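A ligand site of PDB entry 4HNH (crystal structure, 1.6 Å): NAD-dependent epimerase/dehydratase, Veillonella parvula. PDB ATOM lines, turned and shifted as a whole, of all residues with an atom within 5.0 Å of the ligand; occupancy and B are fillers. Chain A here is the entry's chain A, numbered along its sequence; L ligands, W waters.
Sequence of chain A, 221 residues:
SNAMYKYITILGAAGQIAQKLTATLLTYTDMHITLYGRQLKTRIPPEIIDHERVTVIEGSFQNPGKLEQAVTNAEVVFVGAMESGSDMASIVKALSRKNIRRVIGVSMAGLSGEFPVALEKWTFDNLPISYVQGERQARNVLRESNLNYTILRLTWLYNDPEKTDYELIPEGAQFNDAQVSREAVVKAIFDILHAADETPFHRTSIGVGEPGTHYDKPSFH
The backbone NH (N) of Phe 61 lies within hydrogen-bond range of a nitrogen (N4) of the ligand (2.9 Å).
O5 of the ligand sits at hydrogen-bond distance from N of Gly 15 (3.1 Å).
The guanidinium group of Arg 43 is in salt-bridge range of an oxygen (O16) of the ligand (2.7 Å).
OE2 of Glu 83 is in hydrogen-bond range of O12 of the ligand (2.8 Å).
The backbone NH (N) of Ile 17 sits at hydrogen-bond distance from an oxygen (O9) of the ligand (2.9 Å).
The guanidinium group (NH1) of Arg 38 is in salt-bridge range of an oxygen (O15) of the ligand (3.6 Å).
O14 of the ligand is in hydrogen-bond range of N of Leu 157 (2.9 Å).
A nitrogen (N3) of the ligand lies within hydrogen-bond range of the side-chain carboxylate (OD2) of Asp 87, at 3.0 Å.
The side-chain hydroxyl of Tyr 131 is in hydrogen-bond range of an oxygen (O13) of the ligand.
An oxygen (O1) of the ligand is in hydrogen-bond range of the backbone NH (N) of Gln 16, 3.1 Å away.
An oxygen (O8) of the ligand lies within salt-bridge range of the guanidinium group (NE) of Arg 182.
Water W9 lies within hydrogen-bond range of an oxygen (O13) of the ligand and the side-chain carboxylate (OE2) of Glu 83.
Water W15 lies within hydrogen-bond range of the side-chain carboxylate (OE2) of Glu 135 (2.7 Å), an oxygen (O12) of the ligand (2.7 Å), the backbone carbonyl oxygen (O) of Val 106 (2.8 Å) and the backbone NH (N) of Met 82 (2.8 Å).
Water W6 lies within hydrogen-bond range of an oxygen (O9) of the ligand (2.7 Å), the backbone NH (N) of Ala 18 (3.1 Å) and the backbone carbonyl oxygen (O) of Gly 80 (3.5 Å).
Water W3 lies within hydrogen-bond range of N5 of the ligand and N of Arg 38.
Water W4 lies within hydrogen-bond range of OD2 of Asp 87 and N2 of the ligand.
Water W10 lies within hydrogen-bond range of N3 of the ligand (2.9 Å), OG of Ser 60 (3.5 Å) and N of Gln 62 (3.5 Å).
The side-chain amide nitrogen (NE2) of Gln 16 sits close to the guanidinium group (NH2) of Arg 182, 3.4 Å away.
N of Leu 154 lies within hydrogen-bond range of O of Ser 107.
N of Arg 38 is in hydrogen-bond range of O of Gly 59 (3.3 Å).
O of Val 106 sits close to N of Met 82 (3.5 Å).
The side-chain hydroxyl (OH) of Tyr 131 lies within hydrogen-bond range of the side-chain carboxylate (OE2) of Glu 135 (3.2 Å).
OG of Ser 107 sits at hydrogen-bond distance from OE1 of Glu 135, 3.1 Å away.
The side-chain carboxylate (OD1) of Asp 87 sits at hydrogen-bond distance from the side-chain amide nitrogen (NE2) of Gln 62, 2.9 Å away.
OG of Ser 60 sits close to N of Gln 62 (3.2 Å).
O of Gly 12 touches C2 of the ligand (3.99 Å).
Ala 14 touches the ligand.
Ser 60 touches the ligand.
Gly 80 touches the ligand (O to C11, 3.3 Å).
Ala 81 touches the ligand.
Val 106 touches the ligand (CG2 to C11, 3.7 Å).
O of Ser 107 touches C21 of the ligand, at 3.7 Å.
Leu 154 touches the ligand.
Thr 155 touches the ligand (O to C19, 3.4 Å).
Trp 156 touches the ligand (CE3 to O14, 3.5 Å).
Hydrophobic or aromatic side chains that line the ligand: Ile 17, Phe 61, Ala 81, Val 106, Tyr 131, Leu 154, Trp 156 and Leu 157.
21 residues have an atom within 4 Å of the ligand: Gly 12, Ala 14, Gly 15, Gln 16, Ile 17, Arg 38, Arg 43, Ser 60, Phe 61, Gly 80, Ala 81, Glu 83, Asp 87, Val 106, Ser 107, Tyr 131, Leu 154, Thr 155, Trp 156, Leu 157 and Arg 182.
The nearest printed residue that does not touch the ligand is Met 108 (4.04 Å).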
ATOM      1  N   GLY A  12     -19.282 -26.250   0.720  1.00  0.00           N
ATOM      2  CA  GLY A  12     -19.713 -24.992   0.156  1.00  0.00           C
ATOM      3  C   GLY A  12     -21.145 -25.138  -0.311  1.00  0.00           C
ATOM      4  O   GLY A  12     -21.499 -24.734  -1.425  1.00  0.00           O
ATOM      5  N   ALA A  14     -24.029 -23.845   0.159  1.00  0.00           N
ATOM      6  CA  ALA A  14     -24.980 -22.780  -0.138  1.00  0.00           C
ATOM      7  C   ALA A  14     -24.764 -22.189  -1.525  1.00  0.00           C
ATOM      8  O   ALA A  14     -25.523 -21.323  -1.963  1.00  0.00           O
ATOM      9  CB  ALA A  14     -24.934 -21.680   0.923  1.00  0.00           C
ATOM     10  N   GLY A  15     -23.716 -22.676  -2.191  1.00  0.00           N
ATOM     11  CA  GLY A  15     -23.400 -22.192  -3.529  1.00  0.00           C
ATOM     12  C   GLY A  15     -24.514 -22.533  -4.490  1.00  0.00           C
ATOM     13  O   GLY A  15     -25.291 -23.463  -4.256  1.00  0.00           O
ATOM     14  N   GLN A  16     -24.584 -21.788  -5.590  1.00  0.00           N
ATOM     15  CA  GLN A  16     -25.684 -21.954  -6.546  1.00  0.00           C
ATOM     16  C   GLN A  16     -25.705 -23.345  -7.165  1.00  0.00           C
ATOM     17  O   GLN A  16     -26.738 -24.034  -7.180  1.00  0.00           O
ATOM     18  CB  GLN A  16     -25.596 -20.907  -7.647  1.00  0.00           C
ATOM     19  CG  GLN A  16     -26.055 -19.515  -7.214  1.00  0.00           C
ATOM     20  CD  GLN A  16     -26.521 -18.665  -8.388  1.00  0.00           C
ATOM     21  OE1 GLN A  16     -27.516 -18.971  -9.041  1.00  0.00           O
ATOM     22  NE2 GLN A  16     -25.788 -17.599  -8.665  1.00  0.00           N
ATOM     23  N   ILE A  17     -24.553 -23.768  -7.662  1.00  0.00           N
ATOM     24  CA  ILE A  17     -24.452 -25.124  -8.201  1.00  0.00           C
ATOM     25  C   ILE A  17     -24.670 -26.193  -7.127  1.00  0.00           C
ATOM     26  O   ILE A  17     -25.393 -27.160  -7.331  1.00  0.00           O
ATOM     27  CB  ILE A  17     -23.116 -25.349  -8.970  1.00  0.00           C
ATOM     28  CG1 ILE A  17     -23.162 -24.607 -10.309  1.00  0.00           C
ATOM     29  CG2 ILE A  17     -22.858 -26.853  -9.198  1.00  0.00           C
ATOM     30  CD1 ILE A  17     -21.819 -24.586 -11.028  1.00  0.00           C
ATOM     31  N   ALA A  18     -24.025 -26.008  -5.977  1.00  0.00           N
ATOM     32  CA  ALA A  18     -24.180 -26.943  -4.864  1.00  0.00           C
ATOM     33  C   ALA A  18     -25.629 -27.149  -4.449  1.00  0.00           C
ATOM     34  O   ALA A  18     -26.063 -28.281  -4.235  1.00  0.00           O
ATOM     35  CB  ALA A  18     -23.343 -26.468  -3.691  1.00  0.00           C
ATOM     36  N   GLY A  37     -20.990 -25.655   5.176  1.00  0.00           N
ATOM     37  CA  GLY A  37     -20.675 -24.292   4.778  1.00  0.00           C
ATOM     38  C   GLY A  37     -21.072 -23.288   5.818  1.00  0.00           C
ATOM     39  O   GLY A  37     -21.548 -23.645   6.898  1.00  0.00           O
ATOM     40  N   ARG A  38     -20.879 -22.011   5.506  1.00  0.00           N
ATOM     41  CA  ARG A  38     -21.128 -20.955   6.474  1.00  0.00           C
ATOM     42  C   ARG A  38     -22.618 -20.703   6.710  1.00  0.00           C
ATOM     43  O   ARG A  38     -23.358 -20.417   5.760  1.00  0.00           O
ATOM     44  CB  ARG A  38     -20.483 -19.637   6.048  1.00  0.00           C
ATOM     45  CG  ARG A  38     -18.964 -19.650   6.009  1.00  0.00           C
ATOM     46  CD  ARG A  38     -18.459 -18.230   5.814  1.00  0.00           C
ATOM     47  NE  ARG A  38     -17.030 -18.145   5.580  1.00  0.00           N
ATOM     48  CZ  ARG A  38     -16.473 -18.048   4.376  1.00  0.00           C
ATOM     49  NH1 ARG A  38     -17.223 -18.040   3.287  1.00  0.00           N
ATOM     50  NH2 ARG A  38     -15.155 -17.972   4.258  1.00  0.00           N
ATOM     51  N   ARG A  43     -29.619 -20.324   5.867  1.00  0.00           N
ATOM     52  CA  ARG A  43     -29.502 -20.043   4.438  1.00  0.00           C
ATOM     53  C   ARG A  43     -30.160 -21.099   3.545  1.00  0.00           C
ATOM     54  O   ARG A  43     -30.889 -20.754   2.601  1.00  0.00           O
ATOM     55  CB  ARG A  43     -28.024 -19.880   4.044  1.00  0.00           C
ATOM     56  CG  ARG A  43     -27.338 -18.706   4.720  1.00  0.00           C
ATOM     57  CD  ARG A  43     -25.861 -18.753   4.451  1.00  0.00           C
ATOM     58  NE  ARG A  43     -25.553 -18.373   3.067  1.00  0.00           N
ATOM     59  CZ  ARG A  43     -24.346 -18.497   2.543  1.00  0.00           C
ATOM     60  NH1 ARG A  43     -23.373 -19.018   3.280  1.00  0.00           N
ATOM     61  NH2 ARG A  43     -24.109 -18.121   1.286  1.00  0.00           N
ATOM     62  N   GLY A  59     -19.796 -24.391   9.097  1.00  0.00           N
ATOM     63  CA  GLY A  59     -18.393 -24.043   9.304  1.00  0.00           C
ATOM     64  C   GLY A  59     -17.756 -23.496   8.044  1.00  0.00           C
ATOM     65  O   GLY A  59     -18.375 -23.466   6.982  1.00  0.00           O
ATOM     66  N   SER A  60     -16.505 -23.062   8.153  1.00  0.00           N
ATOM     67  CA  SER A  60     -15.798 -22.519   7.002  1.00  0.00           C
ATOM     68  C   SER A  60     -14.714 -23.490   6.547  1.00  0.00           C
ATOM     69  O   SER A  60     -14.351 -24.412   7.278  1.00  0.00           O
ATOM     70  CB  SER A  60     -15.173 -21.167   7.346  1.00  0.00           C
ATOM     71  OG  SER A  60     -13.943 -21.335   8.023  1.00  0.00           O
ATOM     72  N   PHE A  61     -14.204 -23.291   5.337  1.00  0.00           N
ATOM     73  CA  PHE A  61     -13.160 -24.170   4.797  1.00  0.00           C
ATOM     74  C   PHE A  61     -11.884 -24.092   5.627  1.00  0.00           C
ATOM     75  O   PHE A  61     -10.949 -24.844   5.376  1.00  0.00           O
ATOM     76  CB  PHE A  61     -12.823 -23.818   3.335  1.00  0.00           C
ATOM     77  CG  PHE A  61     -13.902 -24.141   2.337  1.00  0.00           C
ATOM     78  CD1 PHE A  61     -15.037 -24.844   2.708  1.00  0.00           C
ATOM     79  CD2 PHE A  61     -13.753 -23.754   1.004  1.00  0.00           C
ATOM     80  CE1 PHE A  61     -16.015 -25.133   1.777  1.00  0.00           C
ATOM     81  CE2 PHE A  61     -14.731 -24.043   0.072  1.00  0.00           C
ATOM     82  CZ  PHE A  61     -15.867 -24.733   0.459  1.00  0.00           C
ATOM     83  N   GLN A  62     -11.829 -23.179   6.579  1.00  0.00           N
ATOM     84  CA  GLN A  62     -10.664 -23.014   7.451  1.00  0.00           C
ATOM     85  C   GLN A  62     -10.890 -23.601   8.846  1.00  0.00           C
ATOM     86  O   GLN A  62     -10.113 -23.330   9.758  1.00  0.00           O
ATOM     87  CB  GLN A  62     -10.267 -21.541   7.565  1.00  0.00           C
ATOM     88  CG  GLN A  62      -9.654 -20.962   6.305  1.00  0.00           C
ATOM     89  CD  GLN A  62      -8.249 -21.479   6.032  1.00  0.00           C
ATOM     90  OE1 GLN A  62      -7.482 -21.758   6.952  1.00  0.00           O
ATOM     91  NE2 GLN A  62      -7.915 -21.627   4.755  1.00  0.00           N
ATOM     92  N   GLY A  80     -17.304 -27.206  -3.838  1.00  0.00           N
ATOM     93  CA  GLY A  80     -18.127 -26.261  -4.568  1.00  0.00           C
ATOM     94  C   GLY A  80     -17.448 -24.968  -4.986  1.00  0.00           C
ATOM     95  O   GLY A  80     -18.037 -24.163  -5.725  1.00  0.00           O
ATOM     96  N   ALA A  81     -16.239 -24.735  -4.483  1.00  0.00           N
ATOM     97  CA  ALA A  81     -15.425 -23.592  -4.880  1.00  0.00           C
ATOM     98  C   ALA A  81     -13.954 -23.977  -4.823  1.00  0.00           C
ATOM     99  O   ALA A  81     -13.513 -24.642  -3.882  1.00  0.00           O
ATOM    100  CB  ALA A  81     -15.702 -22.366  -3.968  1.00  0.00           C
ATOM    101  N   MET A  82     -13.198 -23.567  -5.844  1.00  0.00           N
ATOM    102  CA  MET A  82     -11.753 -23.763  -5.884  1.00  0.00           C
ATOM    103  C   MET A  82     -11.090 -22.420  -6.151  1.00  0.00           C
ATOM    104  O   MET A  82     -10.457 -22.212  -7.185  1.00  0.00           O
ATOM    105  CB  MET A  82     -11.363 -24.794  -6.954  1.00  0.00           C
ATOM    106  CG  MET A  82     -11.774 -26.233  -6.628  1.00  0.00           C
ATOM    107  SD  MET A  82     -11.359 -27.368  -7.970  1.00  0.00           S
ATOM    108  CE  MET A  82      -9.562 -27.314  -7.963  1.00  0.00           C
ATOM    109  N   GLU A  83     -11.239 -21.499  -5.201  1.00  0.00           N
ATOM    110  CA  GLU A  83     -10.832 -20.106  -5.404  1.00  0.00           C
ATOM    111  C   GLU A  83      -9.549 -19.713  -4.666  1.00  0.00           C
ATOM    112  O   GLU A  83      -8.953 -18.692  -4.966  1.00  0.00           O
ATOM    113  CB  GLU A  83     -11.969 -19.198  -4.966  1.00  0.00           C
ATOM    114  CG  GLU A  83     -13.222 -19.359  -5.793  1.00  0.00           C
ATOM    115  CD  GLU A  83     -14.378 -18.552  -5.265  1.00  0.00           C
ATOM    116  OE1 GLU A  83     -14.132 -17.507  -4.622  1.00  0.00           O
ATOM    117  OE2 GLU A  83     -15.543 -18.944  -5.491  1.00  0.00           O
ATOM    118  N   ASP A  87      -7.522 -22.319   1.243  1.00  0.00           N
ATOM    119  CA  ASP A  87      -8.764 -23.033   1.529  1.00  0.00           C
ATOM    120  C   ASP A  87      -8.667 -24.443   0.955  1.00  0.00           C
ATOM    121  O   ASP A  87      -9.084 -25.412   1.602  1.00  0.00           O
ATOM    122  CB  ASP A  87      -9.979 -22.312   0.930  1.00  0.00           C
ATOM    123  CG  ASP A  87     -10.337 -21.034   1.684  1.00  0.00           C
ATOM    124  OD1 ASP A  87      -9.857 -20.841   2.821  1.00  0.00           O
ATOM    125  OD2 ASP A  87     -11.116 -20.222   1.135  1.00  0.00           O
ATOM    126  N   VAL A 106     -15.121 -27.832  -8.656  1.00  0.00           N
ATOM    127  CA  VAL A 106     -15.429 -26.925  -9.766  1.00  0.00           C
ATOM    128  C   VAL A 106     -14.474 -25.735  -9.813  1.00  0.00           C
ATOM    129  O   VAL A 106     -14.235 -25.070  -8.799  1.00  0.00           O
ATOM    130  CB  VAL A 106     -16.907 -26.444  -9.733  1.00  0.00           C
ATOM    131  CG1 VAL A 106     -17.828 -27.576 -10.210  1.00  0.00           C
ATOM    132  CG2 VAL A 106     -17.292 -25.977  -8.364  1.00  0.00           C
ATOM    133  N   SER A 107     -13.917 -25.497 -11.001  1.00  0.00           N
ATOM    134  CA  SER A 107     -12.912 -24.470 -11.236  1.00  0.00           C
ATOM    135  C   SER A 107     -13.342 -23.674 -12.455  1.00  0.00           C
ATOM    136  O   SER A 107     -14.388 -23.958 -13.051  1.00  0.00           O
ATOM    137  CB  SER A 107     -11.541 -25.141 -11.468  1.00  0.00           C
ATOM    138  OG  SER A 107     -10.495 -24.187 -11.708  1.00  0.00           O
ATOM    139  N   MET A 108     -12.566 -22.662 -12.815  1.00  0.00           N
ATOM    140  CA  MET A 108     -12.918 -21.809 -13.948  1.00  0.00           C
ATOM    141  C   MET A 108     -12.146 -22.224 -15.189  1.00  0.00           C
ATOM    142  O   MET A 108     -10.977 -22.554 -15.112  1.00  0.00           O
ATOM    143  CB  MET A 108     -12.594 -20.352 -13.622  1.00  0.00           C
ATOM    144  CG  MET A 108     -11.115 -20.107 -13.420  1.00  0.00           C
ATOM    145  SD  MET A 108     -10.713 -18.362 -13.517  1.00  0.00           S
ATOM    146  CE  MET A 108     -10.771 -18.096 -15.296  1.00  0.00           C
ATOM    147  N   TYR A 131      -8.465 -13.211  -8.629  1.00  0.00           N
ATOM    148  CA  TYR A 131      -9.383 -14.350  -8.658  1.00  0.00           C
ATOM    149  C   TYR A 131      -8.807 -15.445  -9.531  1.00  0.00           C
ATOM    150  O   TYR A 131      -8.809 -16.616  -9.168  1.00  0.00           O
ATOM    151  CB  TYR A 131     -10.763 -13.919  -9.190  1.00  0.00           C
ATOM    152  CG  TYR A 131     -11.735 -15.051  -9.392  1.00  0.00           C
ATOM    153  CD1 TYR A 131     -12.555 -15.501  -8.355  1.00  0.00           C
ATOM    154  CD2 TYR A 131     -11.853 -15.678 -10.619  1.00  0.00           C
ATOM    155  CE1 TYR A 131     -13.439 -16.534  -8.553  1.00  0.00           C
ATOM    156  CE2 TYR A 131     -12.727 -16.716 -10.826  1.00  0.00           C
ATOM    157  CZ  TYR A 131     -13.531 -17.136  -9.787  1.00  0.00           C
ATOM    158  OH  TYR A 131     -14.408 -18.170 -10.021  1.00  0.00           O
ATOM    159  N   GLU A 135      -7.568 -19.187  -8.373  1.00  0.00           N
ATOM    160  CA  GLU A 135      -8.059 -20.408  -8.979  1.00  0.00           C
ATOM    161  C   GLU A 135      -6.898 -21.282  -9.429  1.00  0.00           C
ATOM    162  O   GLU A 135      -6.948 -22.515  -9.297  1.00  0.00           O
ATOM    163  CB  GLU A 135      -8.983 -20.090 -10.151  1.00  0.00           C
ATOM    164  CG  GLU A 135     -10.328 -19.490  -9.723  1.00  0.00           C
ATOM    165  CD  GLU A 135     -11.428 -20.541  -9.575  1.00  0.00           C
ATOM    166  OE1 GLU A 135     -11.350 -21.590 -10.227  1.00  0.00           O
ATOM    167  OE2 GLU A 135     -12.376 -20.316  -8.777  1.00  0.00           O
ATOM    168  N   LEU A 154     -15.353 -24.904 -15.562  1.00  0.00           N
ATOM    169  CA  LEU A 154     -16.613 -24.353 -16.005  1.00  0.00           C
ATOM    170  C   LEU A 154     -16.436 -23.057 -16.763  1.00  0.00           C
ATOM    171  O   LEU A 154     -15.677 -22.163 -16.349  1.00  0.00           O
ATOM    172  CB  LEU A 154     -17.566 -24.119 -14.834  1.00  0.00           C
ATOM    173  CG  LEU A 154     -17.775 -25.302 -13.873  1.00  0.00           C
ATOM    174  CD1 LEU A 154     -18.754 -24.932 -12.784  1.00  0.00           C
ATOM    175  CD2 LEU A 154     -18.199 -26.574 -14.627  1.00  0.00           C
ATOM    176  N   THR A 155     -17.144 -22.932 -17.878  1.00  0.00           N
ATOM    177  CA  THR A 155     -17.192 -21.661 -18.576  1.00  0.00           C
ATOM    178  C   THR A 155     -18.228 -20.769 -17.906  1.00  0.00           C
ATOM    179  O   THR A 155     -18.720 -21.092 -16.827  1.00  0.00           O
ATOM    180  CB  THR A 155     -17.403 -21.869 -20.082  1.00  0.00           C
ATOM    181  OG1 THR A 155     -17.324 -20.619 -20.758  1.00  0.00           O
ATOM    182  CG2 THR A 155     -18.744 -22.537 -20.367  1.00  0.00           C
ATOM    183  N   TRP A 156     -18.533 -19.626 -18.502  1.00  0.00           N
ATOM    184  CA  TRP A 156     -19.389 -18.652 -17.825  1.00  0.00           C
ATOM    185  C   TRP A 156     -20.782 -19.206 -17.492  1.00  0.00           C
ATOM    186  O   TRP A 156     -21.428 -19.836 -18.322  1.00  0.00           O
ATOM    187  CB  TRP A 156     -19.517 -17.376 -18.643  1.00  0.00           C
ATOM    188  CG  TRP A 156     -18.259 -16.590 -18.694  1.00  0.00           C
ATOM    189  CD1 TRP A 156     -17.265 -16.653 -19.642  1.00  0.00           C
ATOM    190  CD2 TRP A 156     -17.843 -15.588 -17.757  1.00  0.00           C
ATOM    191  NE1 TRP A 156     -16.272 -15.754 -19.348  1.00  0.00           N
ATOM    192  CE2 TRP A 156     -16.592 -15.083 -18.197  1.00  0.00           C
ATOM    193  CE3 TRP A 156     -18.413 -15.063 -16.593  1.00  0.00           C
ATOM    194  CZ2 TRP A 156     -15.899 -14.084 -17.500  1.00  0.00           C
ATOM    195  CZ3 TRP A 156     -17.730 -14.077 -15.911  1.00  0.00           C
ATOM    196  CH2 TRP A 156     -16.496 -13.595 -16.359  1.00  0.00           C
ATOM    197  N   LEU A 157     -21.228 -18.944 -16.270  1.00  0.00           N
ATOM    198  CA  LEU A 157     -22.459 -19.554 -15.772  1.00  0.00           C
ATOM    199  C   LEU A 157     -23.694 -18.663 -15.870  1.00  0.00           C
ATOM    200  O   LEU A 157     -23.601 -17.433 -15.706  1.00  0.00           O
ATOM    201  CB  LEU A 157     -22.291 -19.959 -14.298  1.00  0.00           C
ATOM    202  CG  LEU A 157     -21.203 -20.998 -14.003  1.00  0.00           C
ATOM    203  CD1 LEU A 157     -21.005 -21.167 -12.483  1.00  0.00           C
ATOM    204  CD2 LEU A 157     -21.538 -22.329 -14.643  1.00  0.00           C
ATOM    205  N   ARG A 182     -26.096 -23.497 -15.031  1.00  0.00           N
ATOM    206  CA  ARG A 182     -25.775 -24.236 -13.810  1.00  0.00           C
ATOM    207  C   ARG A 182     -26.514 -25.588 -13.779  1.00  0.00           C
ATOM    208  O   ARG A 182     -25.997 -26.557 -13.246  1.00  0.00           O
ATOM    209  CB  ARG A 182     -26.093 -23.397 -12.575  1.00  0.00           C
ATOM    210  CG  ARG A 182     -25.129 -22.233 -12.412  1.00  0.00           C
ATOM    211  CD  ARG A 182     -25.377 -21.499 -11.117  1.00  0.00           C
ATOM    212  NE  ARG A 182     -24.433 -20.409 -10.961  1.00  0.00           N
ATOM    213  CZ  ARG A 182     -24.631 -19.190 -11.472  1.00  0.00           C
ATOM    214  NH1 ARG A 182     -25.734 -18.936 -12.172  1.00  0.00           N
ATOM    215  NH2 ARG A 182     -23.725 -18.239 -11.286  1.00  0.00           N
HETATM  216  P1  LIG L   1     -21.088 -19.825  -5.763  1.00  0.00           P
HETATM  217  O1  LIG L   1     -22.545 -19.501  -5.772  1.00  0.00           O
HETATM  218  O2  LIG L   1     -20.393 -18.566  -5.343  1.00  0.00           O
HETATM  219  O3  LIG L   1     -20.791 -20.969  -4.723  1.00  0.00           O
HETATM  220  C1  LIG L   1     -19.525 -21.066  -4.113  1.00  0.00           C
HETATM  221  C2  LIG L   1     -19.705 -21.405  -2.692  1.00  0.00           C
HETATM  222  O4  LIG L   1     -18.444 -21.758  -2.112  1.00  0.00           O
HETATM  223  C3  LIG L   1     -20.277 -20.246  -1.919  1.00  0.00           C
HETATM  224  O5  LIG L   1     -21.519 -20.572  -1.401  1.00  0.00           O
HETATM  225  C4  LIG L   1     -19.262 -20.004  -0.861  1.00  0.00           C
HETATM  226  O6  LIG L   1     -19.804 -19.749   0.426  1.00  0.00           O
HETATM  227  C5  LIG L   1     -18.508 -21.302  -0.809  1.00  0.00           C
HETATM  228  N1  LIG L   1     -17.206 -21.063  -0.256  1.00  0.00           N
HETATM  229  C6  LIG L   1     -16.087 -20.520  -0.908  1.00  0.00           C
HETATM  230  N2  LIG L   1     -15.096 -20.410  -0.028  1.00  0.00           N
HETATM  231  C7  LIG L   1     -15.523 -20.877   1.229  1.00  0.00           C
HETATM  232  C8  LIG L   1     -14.923 -20.997   2.526  1.00  0.00           C
HETATM  233  N3  LIG L   1     -13.597 -20.616   2.729  1.00  0.00           N
HETATM  234  N4  LIG L   1     -15.670 -21.483   3.530  1.00  0.00           N
HETATM  235  C9  LIG L   1     -16.924 -21.858   3.350  1.00  0.00           C
HETATM  236  N5  LIG L   1     -17.543 -21.767   2.151  1.00  0.00           N
HETATM  237  C10 LIG L   1     -16.881 -21.286   1.097  1.00  0.00           C
HETATM  238  O7  LIG L   1     -20.539 -20.256  -7.179  1.00  0.00           O
HETATM  239  P2  LIG L   1     -21.254 -21.225  -8.242  1.00  0.00           P
HETATM  240  O8  LIG L   1     -22.178 -20.507  -9.168  1.00  0.00           O
HETATM  241  O9  LIG L   1     -22.104 -22.299  -7.647  1.00  0.00           O
HETATM  242  O10 LIG L   1     -20.054 -21.804  -9.098  1.00  0.00           O
HETATM  243  C11 LIG L   1     -19.153 -22.729  -8.494  1.00  0.00           C
HETATM  244  C12 LIG L   1     -17.701 -22.218  -8.538  1.00  0.00           C
HETATM  245  O11 LIG L   1     -17.236 -22.036  -9.838  1.00  0.00           O
HETATM  246  C13 LIG L   1     -17.455 -20.919  -7.800  1.00  0.00           C
HETATM  247  O12 LIG L   1     -16.209 -20.977  -7.234  1.00  0.00           O
HETATM  248  C14 LIG L   1     -17.503 -19.913  -8.901  1.00  0.00           C
HETATM  249  O13 LIG L   1     -16.820 -18.758  -8.577  1.00  0.00           O
HETATM  250  C15 LIG L   1     -16.816 -20.694  -9.962  1.00  0.00           C
HETATM  251  N6  LIG L   1     -17.122 -20.282 -11.359  1.00  0.00           N
HETATM  252  C16 LIG L   1     -17.978 -19.217 -11.614  1.00  0.00           C
HETATM  253  C17 LIG L   1     -18.270 -18.850 -12.924  1.00  0.00           C
HETATM  254  C18 LIG L   1     -19.167 -17.724 -13.190  1.00  0.00           C
HETATM  255  O14 LIG L   1     -19.554 -17.517 -14.318  1.00  0.00           O
HETATM  256  N7  LIG L   1     -19.609 -16.881 -12.115  1.00  0.00           N
HETATM  257  C19 LIG L   1     -17.689 -19.610 -13.995  1.00  0.00           C
HETATM  258  C20 LIG L   1     -16.801 -20.716 -13.669  1.00  0.00           C
HETATM  259  C21 LIG L   1     -16.560 -21.015 -12.375  1.00  0.00           C
HETATM  260  P3  LIG L   1     -20.401 -18.368   0.899  1.00  0.00           P
HETATM  261  O15 LIG L   1     -19.524 -17.139   0.692  1.00  0.00           O
HETATM  262  O16 LIG L   1     -21.687 -18.068   0.143  1.00  0.00           O
HETATM  263  O17 LIG L   1     -20.721 -18.411   2.389  1.00  0.00           O
HETATM  264  O   HOH W   1     -23.698 -17.889  -4.121  1.00  0.00           O
HETATM  265  O   HOH W   2     -21.545 -22.427   0.836  1.00  0.00           O
HETATM  266  O   HOH W   3     -20.149 -21.238   2.936  1.00  0.00           O
HETATM  267  O   HOH W   4     -12.405 -20.491  -0.953  1.00  0.00           O
HETATM  268  O   HOH W   5     -19.277 -13.610 -12.285  1.00  0.00           O
HETATM  269  O   HOH W   6     -21.533 -24.179  -5.746  1.00  0.00           O
HETATM  270  O   HOH W   7     -21.832 -14.861   1.346  1.00  0.00           O
HETATM  271  O   HOH W   8     -16.998 -18.477  -3.103  1.00  0.00           O
HETATM  272  O   HOH W   9     -18.092 -17.333  -6.723  1.00  0.00           O
HETATM  273  O   HOH W  10     -12.357 -20.018   5.231  1.00  0.00           O
HETATM  274  O   HOH W  11     -21.506 -15.746 -14.255  1.00  0.00           O
HETATM  275  O   HOH W  12     -20.924 -18.194  -9.898  1.00  0.00           O
HETATM  276  O   HOH W  13     -20.976 -16.424   4.052  1.00  0.00           O
HETATM  277  O   HOH W  14     -22.471 -16.834  -1.836  1.00  0.00           O
HETATM  278  O   HOH W  15     -14.068 -22.359  -8.212  1.00  0.00           O
